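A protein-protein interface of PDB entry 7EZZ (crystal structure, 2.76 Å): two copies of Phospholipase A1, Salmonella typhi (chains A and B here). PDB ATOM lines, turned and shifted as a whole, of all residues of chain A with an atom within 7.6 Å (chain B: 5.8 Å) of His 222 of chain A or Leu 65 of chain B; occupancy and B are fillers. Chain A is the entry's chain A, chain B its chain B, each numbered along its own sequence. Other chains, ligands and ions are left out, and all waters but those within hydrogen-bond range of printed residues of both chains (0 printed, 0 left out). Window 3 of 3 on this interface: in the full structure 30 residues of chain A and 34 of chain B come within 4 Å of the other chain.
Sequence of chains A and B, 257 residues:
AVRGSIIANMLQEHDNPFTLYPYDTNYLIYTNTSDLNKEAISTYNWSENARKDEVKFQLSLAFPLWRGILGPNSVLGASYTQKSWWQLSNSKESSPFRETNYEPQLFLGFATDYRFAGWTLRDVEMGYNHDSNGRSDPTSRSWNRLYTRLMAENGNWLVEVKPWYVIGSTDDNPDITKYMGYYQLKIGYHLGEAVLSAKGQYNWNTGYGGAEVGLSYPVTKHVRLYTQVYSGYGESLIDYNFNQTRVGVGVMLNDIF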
ATOM      1  N   PRO A 218      10.961  25.996  10.220  1.00  0.00           N
ATOM      2  CA  PRO A 218      10.003  25.405   9.277  1.00  0.00           C
ATOM      3  C   PRO A 218       9.506  24.099   9.894  1.00  0.00           C
ATOM      4  O   PRO A 218      10.318  23.233  10.237  1.00  0.00           O
ATOM      5  CB  PRO A 218      10.840  25.105   8.020  1.00  0.00           C
ATOM      6  CG  PRO A 218      12.273  25.044   8.523  1.00  0.00           C
ATOM      7  CD  PRO A 218      12.353  25.956   9.731  1.00  0.00           C
ATOM      8  N   VAL A 219       8.182  24.009  10.086  1.00  0.00           N
ATOM      9  CA  VAL A 219       7.500  22.798  10.525  1.00  0.00           C
ATOM     10  C   VAL A 219       7.124  22.018   9.266  1.00  0.00           C
ATOM     11  O   VAL A 219       7.147  20.790   9.233  1.00  0.00           O
ATOM     12  CB  VAL A 219       6.255  23.134  11.379  1.00  0.00           C
ATOM     13  CG1 VAL A 219       5.551  21.891  11.894  1.00  0.00           C
ATOM     14  CG2 VAL A 219       6.586  24.033  12.556  1.00  0.00           C
ATOM     15  N   THR A 220       6.803  22.770   8.212  1.00  0.00           N
ATOM     16  CA  THR A 220       6.553  22.223   6.894  1.00  0.00           C
ATOM     17  C   THR A 220       7.109  23.193   5.866  1.00  0.00           C
ATOM     18  O   THR A 220       7.705  24.220   6.206  1.00  0.00           O
ATOM     19  CB  THR A 220       5.052  22.055   6.629  1.00  0.00           C
ATOM     20  OG1 THR A 220       4.393  23.310   6.392  1.00  0.00           O
ATOM     21  CG2 THR A 220       4.352  21.267   7.720  1.00  0.00           C
ATOM     22  N   LYS A 221       6.923  22.829   4.596  1.00  0.00           N
ATOM     23  CA  LYS A 221       7.358  23.679   3.497  1.00  0.00           C
ATOM     24  C   LYS A 221       6.350  24.806   3.281  1.00  0.00           C
ATOM     25  O   LYS A 221       6.414  25.493   2.277  1.00  0.00           O
ATOM     26  CB  LYS A 221       7.519  22.840   2.226  1.00  0.00           C
ATOM     27  CG  LYS A 221       8.520  21.700   2.323  1.00  0.00           C
ATOM     28  CD  LYS A 221       8.744  21.007   1.007  1.00  0.00           C
ATOM     29  CE  LYS A 221       9.943  20.086   1.043  1.00  0.00           C
ATOM     30  NZ  LYS A 221      10.232  19.528  -0.299  1.00  0.00           N
ATOM     31  N   HIS A 222       5.413  24.983   4.219  1.00  0.00           N
ATOM     32  CA  HIS A 222       4.344  25.967   4.101  1.00  0.00           C
ATOM     33  C   HIS A 222       4.289  26.865   5.334  1.00  0.00           C
ATOM     34  O   HIS A 222       4.113  28.074   5.259  1.00  0.00           O
ATOM     35  CB  HIS A 222       3.018  25.236   3.859  1.00  0.00           C
ATOM     36  CG  HIS A 222       2.941  24.606   2.505  1.00  0.00           C
ATOM     37  ND1 HIS A 222       2.592  23.281   2.324  1.00  0.00           N
ATOM     38  CD2 HIS A 222       3.216  25.104   1.273  1.00  0.00           C
ATOM     39  CE1 HIS A 222       2.625  23.000   1.036  1.00  0.00           C
ATOM     40  NE2 HIS A 222       3.002  24.100   0.368  1.00  0.00           N
ATOM     41  N   VAL A 223       4.507  26.246   6.483  1.00  0.00           N
ATOM     42  CA  VAL A 223       4.303  26.925   7.745  1.00  0.00           C
ATOM     43  C   VAL A 223       5.589  26.831   8.574  1.00  0.00           C
ATOM     44  O   VAL A 223       6.215  25.763   8.653  1.00  0.00           O
ATOM     45  CB  VAL A 223       3.068  26.330   8.461  1.00  0.00           C
ATOM     46  CG1 VAL A 223       2.718  27.081   9.724  1.00  0.00           C
ATOM     47  CG2 VAL A 223       1.857  26.336   7.540  1.00  0.00           C
ATOM     48  N   ARG A 224       5.953  27.972   9.192  1.00  0.00           N
ATOM     49  CA  ARG A 224       6.985  27.985  10.215  1.00  0.00           C
ATOM     50  C   ARG A 224       6.331  28.140  11.584  1.00  0.00           C
ATOM     51  O   ARG A 224       5.375  28.919  11.738  1.00  0.00           O
ATOM     52  CB  ARG A 224       7.989  29.129  10.007  1.00  0.00           C
ATOM     53  CG  ARG A 224       8.709  29.121   8.669  1.00  0.00           C
ATOM     54  CD  ARG A 224       9.599  30.346   8.439  1.00  0.00           C
ATOM     55  NE  ARG A 224      10.812  30.308   9.261  1.00  0.00           N
ATOM     56  CZ  ARG A 224      11.910  29.635   8.934  1.00  0.00           C
ATOM     57  NH1 ARG A 224      11.944  28.956   7.801  1.00  0.00           N
ATOM     58  NH2 ARG A 224      12.951  29.619   9.747  1.00  0.00           N
ATOM     59  N   VAL A 251       2.251  30.890  14.160  1.00  0.00           N
ATOM     60  CA  VAL A 251       2.741  30.454  12.856  1.00  0.00           C
ATOM     61  C   VAL A 251       3.240  31.643  12.047  1.00  0.00           C
ATOM     62  O   VAL A 251       2.823  32.786  12.276  1.00  0.00           O
ATOM     63  CB  VAL A 251       1.682  29.662  12.078  1.00  0.00           C
ATOM     64  CG1 VAL A 251       1.428  28.302  12.716  1.00  0.00           C
ATOM     65  CG2 VAL A 251       0.383  30.452  11.971  1.00  0.00           C
ATOM     66  N   MET A 252       4.155  31.346  11.104  1.00  0.00           N
ATOM     67  CA  MET A 252       4.786  32.375  10.295  1.00  0.00           C
ATOM     68  C   MET A 252       4.950  31.867   8.864  1.00  0.00           C
ATOM     69  O   MET A 252       5.194  30.676   8.677  1.00  0.00           O
ATOM     70  CB  MET A 252       6.146  32.715  10.911  1.00  0.00           C
ATOM     71  CG  MET A 252       7.015  33.650  10.098  1.00  0.00           C
ATOM     72  SD  MET A 252       8.656  33.810  10.867  1.00  0.00           S
ATOM     73  CE  MET A 252       8.429  35.361  11.740  1.00  0.00           C
ATOM     74  N   LEU A 253       4.795  32.760   7.872  1.00  0.00           N
ATOM     75  CA  LEU A 253       5.144  32.404   6.507  1.00  0.00           C
ATOM     76  C   LEU A 253       6.633  32.605   6.277  1.00  0.00           C
ATOM     77  O   LEU A 253       7.341  31.651   6.004  1.00  0.00           O
ATOM     78  CB  LEU A 253       4.404  33.295   5.521  1.00  0.00           C
ATOM     79  CG  LEU A 253       2.899  33.214   5.565  1.00  0.00           C
ATOM     80  CD1 LEU A 253       2.341  34.125   4.472  1.00  0.00           C
ATOM     81  CD2 LEU A 253       2.479  31.766   5.365  1.00  0.00           C
ATOM     82  N   ASN A 254       7.071  33.862   6.331  1.00  0.00           N
ATOM     83  CA  ASN A 254       8.438  34.251   6.043  1.00  0.00           C
ATOM     84  C   ASN A 254       9.047  34.906   7.289  1.00  0.00           C
ATOM     85  O   ASN A 254       8.373  35.579   8.087  1.00  0.00           O
ATOM     86  CB  ASN A 254       8.504  35.124   4.784  1.00  0.00           C
ATOM     87  CG  ASN A 254       7.767  36.438   4.951  1.00  0.00           C
ATOM     88  OD1 ASN A 254       6.559  36.461   5.165  1.00  0.00           O
ATOM     89  ND2 ASN A 254       8.488  37.546   4.893  1.00  0.00           N
ATOM     90  N   MET B  10      -2.182  27.707  -6.231  1.00  0.00           N
ATOM     91  CA  MET B  10      -1.777  27.221  -4.920  1.00  0.00           C
ATOM     92  C   MET B  10      -1.004  25.910  -5.010  1.00  0.00           C
ATOM     93  O   MET B  10      -0.243  25.611  -4.093  1.00  0.00           O
ATOM     94  CB  MET B  10      -2.989  27.017  -4.016  1.00  0.00           C
ATOM     95  CG  MET B  10      -3.363  28.266  -3.296  1.00  0.00           C
ATOM     96  SD  MET B  10      -4.568  27.906  -2.038  1.00  0.00           S
ATOM     97  CE  MET B  10      -6.001  28.519  -2.910  1.00  0.00           C
ATOM     98  N   PHE B  63      -3.064  30.684   1.479  1.00  0.00           N
ATOM     99  CA  PHE B  63      -1.958  30.037   2.167  1.00  0.00           C
ATOM    100  C   PHE B  63      -2.079  28.533   2.025  1.00  0.00           C
ATOM    101  O   PHE B  63      -2.905  27.912   2.693  1.00  0.00           O
ATOM    102  CB  PHE B  63      -1.968  30.339   3.659  1.00  0.00           C
ATOM    103  CG  PHE B  63      -2.119  31.791   4.008  1.00  0.00           C
ATOM    104  CD1 PHE B  63      -1.079  32.685   3.781  1.00  0.00           C
ATOM    105  CD2 PHE B  63      -3.287  32.254   4.594  1.00  0.00           C
ATOM    106  CE1 PHE B  63      -1.199  34.027   4.125  1.00  0.00           C
ATOM    107  CE2 PHE B  63      -3.386  33.591   4.962  1.00  0.00           C
ATOM    108  CZ  PHE B  63      -2.354  34.479   4.720  1.00  0.00           C
ATOM    109  N   PRO B  64      -1.245  27.914   1.152  1.00  0.00           N
ATOM    110  CA  PRO B  64      -1.208  26.457   1.007  1.00  0.00           C
ATOM    111  C   PRO B  64      -0.672  25.863   2.300  1.00  0.00           C
ATOM    112  O   PRO B  64       0.424  26.201   2.734  1.00  0.00           O
ATOM    113  CB  PRO B  64      -0.238  26.214  -0.167  1.00  0.00           C
ATOM    114  CG  PRO B  64      -0.248  27.526  -0.891  1.00  0.00           C
ATOM    115  CD  PRO B  64      -0.323  28.569   0.215  1.00  0.00           C
ATOM    116  N   LEU B  65      -1.487  25.013   2.934  1.00  0.00           N
ATOM    117  CA  LEU B  65      -1.056  24.330   4.144  1.00  0.00           C
ATOM    118  C   LEU B  65      -0.611  22.913   3.800  1.00  0.00           C
ATOM    119  O   LEU B  65       0.393  22.454   4.327  1.00  0.00           O
ATOM    120  CB  LEU B  65      -2.160  24.333   5.207  1.00  0.00           C
ATOM    121  CG  LEU B  65      -2.744  25.698   5.588  1.00  0.00           C
ATOM    122  CD1 LEU B  65      -3.985  25.511   6.449  1.00  0.00           C
ATOM    123  CD2 LEU B  65      -1.721  26.575   6.296  1.00  0.00           C
ATOM    124  N   TRP B  66      -1.322  22.231   2.895  1.00  0.00           N
ATOM    125  CA  TRP B  66      -1.019  20.835   2.607  1.00  0.00           C
ATOM    126  C   TRP B  66      -1.482  20.472   1.196  1.00  0.00           C
ATOM    127  O   TRP B  66      -2.649  20.169   0.967  1.00  0.00           O
ATOM    128  CB  TRP B  66      -1.645  19.944   3.689  1.00  0.00           C
ATOM    129  CG  TRP B  66      -1.411  18.464   3.617  1.00  0.00           C
ATOM    130  CD1 TRP B  66      -0.878  17.728   2.598  1.00  0.00           C
ATOM    131  CD2 TRP B  66      -1.799  17.512   4.625  1.00  0.00           C
ATOM    132  NE1 TRP B  66      -0.862  16.400   2.916  1.00  0.00           N
ATOM    133  CE2 TRP B  66      -1.432  16.236   4.151  1.00  0.00           C
ATOM    134  CE3 TRP B  66      -2.388  17.622   5.893  1.00  0.00           C
ATOM    135  CZ2 TRP B  66      -1.668  15.076   4.893  1.00  0.00           C
ATOM    136  CZ3 TRP B  66      -2.604  16.482   6.632  1.00  0.00           C
ATOM    137  CH2 TRP B  66      -2.266  15.224   6.125  1.00  0.00           C
ATOM    138  N   ARG B  67      -0.540  20.478   0.248  1.00  0.00           N
ATOM    139  CA  ARG B  67      -0.767  20.003  -1.104  1.00  0.00           C
ATOM    140  C   ARG B  67      -0.861  18.477  -1.142  1.00  0.00           C
ATOM    141  O   ARG B  67      -0.062  17.799  -0.528  1.00  0.00           O
ATOM    142  CB  ARG B  67       0.438  20.405  -1.957  1.00  0.00           C
ATOM    143  CG  ARG B  67       0.692  21.901  -1.998  1.00  0.00           C
ATOM    144  CD  ARG B  67       1.768  22.132  -3.020  1.00  0.00           C
ATOM    145  NE  ARG B  67       1.837  23.549  -3.324  1.00  0.00           N
ATOM    146  CZ  ARG B  67       2.859  24.336  -3.018  1.00  0.00           C
ATOM    147  NH1 ARG B  67       3.926  23.839  -2.408  1.00  0.00           N
ATOM    148  NH2 ARG B  67       2.795  25.621  -3.331  1.00  0.00           N
ATOM    149  N   VAL B  75      -5.804  20.428  -2.289  1.00  0.00           N
ATOM    150  CA  VAL B  75      -5.017  21.214  -1.357  1.00  0.00           C
ATOM    151  C   VAL B  75      -5.849  21.600  -0.140  1.00  0.00           C
ATOM    152  O   VAL B  75      -7.006  21.978  -0.254  1.00  0.00           O
ATOM    153  CB  VAL B  75      -4.382  22.440  -2.047  1.00  0.00           C
ATOM    154  CG1 VAL B  75      -5.418  23.485  -2.456  1.00  0.00           C
ATOM    155  CG2 VAL B  75      -3.280  23.048  -1.204  1.00  0.00           C
ATOM    156  N   LEU B  76      -5.205  21.523   1.012  1.00  0.00           N
ATOM    157  CA  LEU B  76      -5.723  22.037   2.292  1.00  0.00           C
ATOM    158  C   LEU B  76      -5.229  23.478   2.299  1.00  0.00           C
ATOM    159  O   LEU B  76      -4.071  23.679   2.124  1.00  0.00           O
ATOM    160  CB  LEU B  76      -5.078  21.243   3.424  1.00  0.00           C
ATOM    161  CG  LEU B  76      -5.749  21.288   4.791  1.00  0.00           C
ATOM    162  CD1 LEU B  76      -4.727  21.454   5.878  1.00  0.00           C
ATOM    163  CD2 LEU B  76      -6.787  22.371   4.892  1.00  0.00           C
ATOM    164  N   GLY B  77      -6.105  24.452   2.410  1.00  0.00           N
ATOM    165  CA  GLY B  77      -5.585  25.815   2.371  1.00  0.00           C
ATOM    166  C   GLY B  77      -6.325  26.745   3.281  1.00  0.00           C
ATOM    167  O   GLY B  77      -7.324  26.391   3.842  1.00  0.00           O
ATOM    168  N   ALA B  78      -5.773  27.921   3.413  1.00  0.00           N
ATOM    169  CA  ALA B  78      -6.374  28.985   4.194  1.00  0.00           C
ATOM    170  C   ALA B  78      -6.301  30.256   3.349  1.00  0.00           C
ATOM    171  O   ALA B  78      -5.458  30.373   2.460  1.00  0.00           O
ATOM    172  CB  ALA B  78      -5.644  29.105   5.516  1.00  0.00           C
ATOM    173  N   LEU B 106     -10.883  28.586   5.986  1.00  0.00           N
ATOM    174  CA  LEU B 106     -10.163  27.317   5.930  1.00  0.00           C
ATOM    175  C   LEU B 106     -10.920  26.390   4.978  1.00  0.00           C
ATOM    176  O   LEU B 106     -12.140  26.286   5.067  1.00  0.00           O
ATOM    177  CB  LEU B 106     -10.078  26.765   7.361  1.00  0.00           C
ATOM    178  CG  LEU B 106      -9.415  25.393   7.533  1.00  0.00           C
ATOM    179  CD1 LEU B 106      -7.935  25.452   7.184  1.00  0.00           C
ATOM    180  CD2 LEU B 106      -9.608  24.830   8.933  1.00  0.00           C
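ND1 of His 222 of chain A sits at hydrogen-bond distance from O of Leu 65 of chain B, 3.1 Å away.
The guanidinium group (NH1) of Arg 67 of chain B is in hydrogen-bond range of a ring nitrogen (NE2) of His 222 of chain A (2.9 Å).
OG1 of Thr 220 of chain A sits at hydrogen-bond distance from N of His 222 of chain A (2.9 Å).
N of Val 223 of chain A sits at hydrogen-bond distance from OG1 of Thr 220 of chain A (2.9 Å).
The backbone carbonyl oxygen of Met 10 of chain B is in hydrogen-bond range of the guanidinium group of Arg 67 of chain B, 3.0 Å away.
The backbone carbonyl oxygen of Ala 78 of chain B is in hydrogen-bond range of the backbone NH of Phe 63 of chain B (2.6 Å).
The backbone NH (N) of Leu 65 of chain B is in hydrogen-bond range of the backbone carbonyl oxygen (O) of Leu 76 of chain B, 3.0 Å away.
Among the printed residues, merely in contact across the chains: His 222 of chain A with Pro 64 of chain B, Leu 253 of chain A with Phe 63 of chain B and Val 223 of chain A with Leu 65 of chain B.
Pro 218 of chain A touches none of the printed residues of chain B.
Of chain B, only Pro 64, Leu 65 and Arg 67 come within 4 Å of His 222 of chain A.
Of the printed residues of chain B, Val 223 of chain A touches Leu 65 (3.8 Å).
Of the printed residues of chain B, Leu 253 of chain A touches Phe 63.
Printed residues of chain A within 4 Å of Leu 65 of chain B: His 222 and Val 223.
The nearest printed residue of chain A that does not touch Phe 63 of chain B is His 222 of chain A (6.3 Å).
Of the 11 printed residues of chain B, 4 touch a printed residue of chain A.
Printed residues of chain B that touch a printed residue of chain A: Phe 63, Pro 64, Leu 65 and Arg 67.
Hydrophobic or aromatic side chains of chain B within 4 Å of the printed part of chain A: Phe 63, Pro 64 and Leu 65.
Printed residues of chain A that touch a printed residue of chain B: His 222, Val 223 and Leu 253.
Among the printed residues, no Asp or Glu carboxylate lies within 4 Å of a Lys or Arg side-chain nitrogen of the other chain.
No position is printed for both chains.
Of the 5 pairs that touch across the chains among the printed residues, none has its exchanged pair printed and touching as well.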
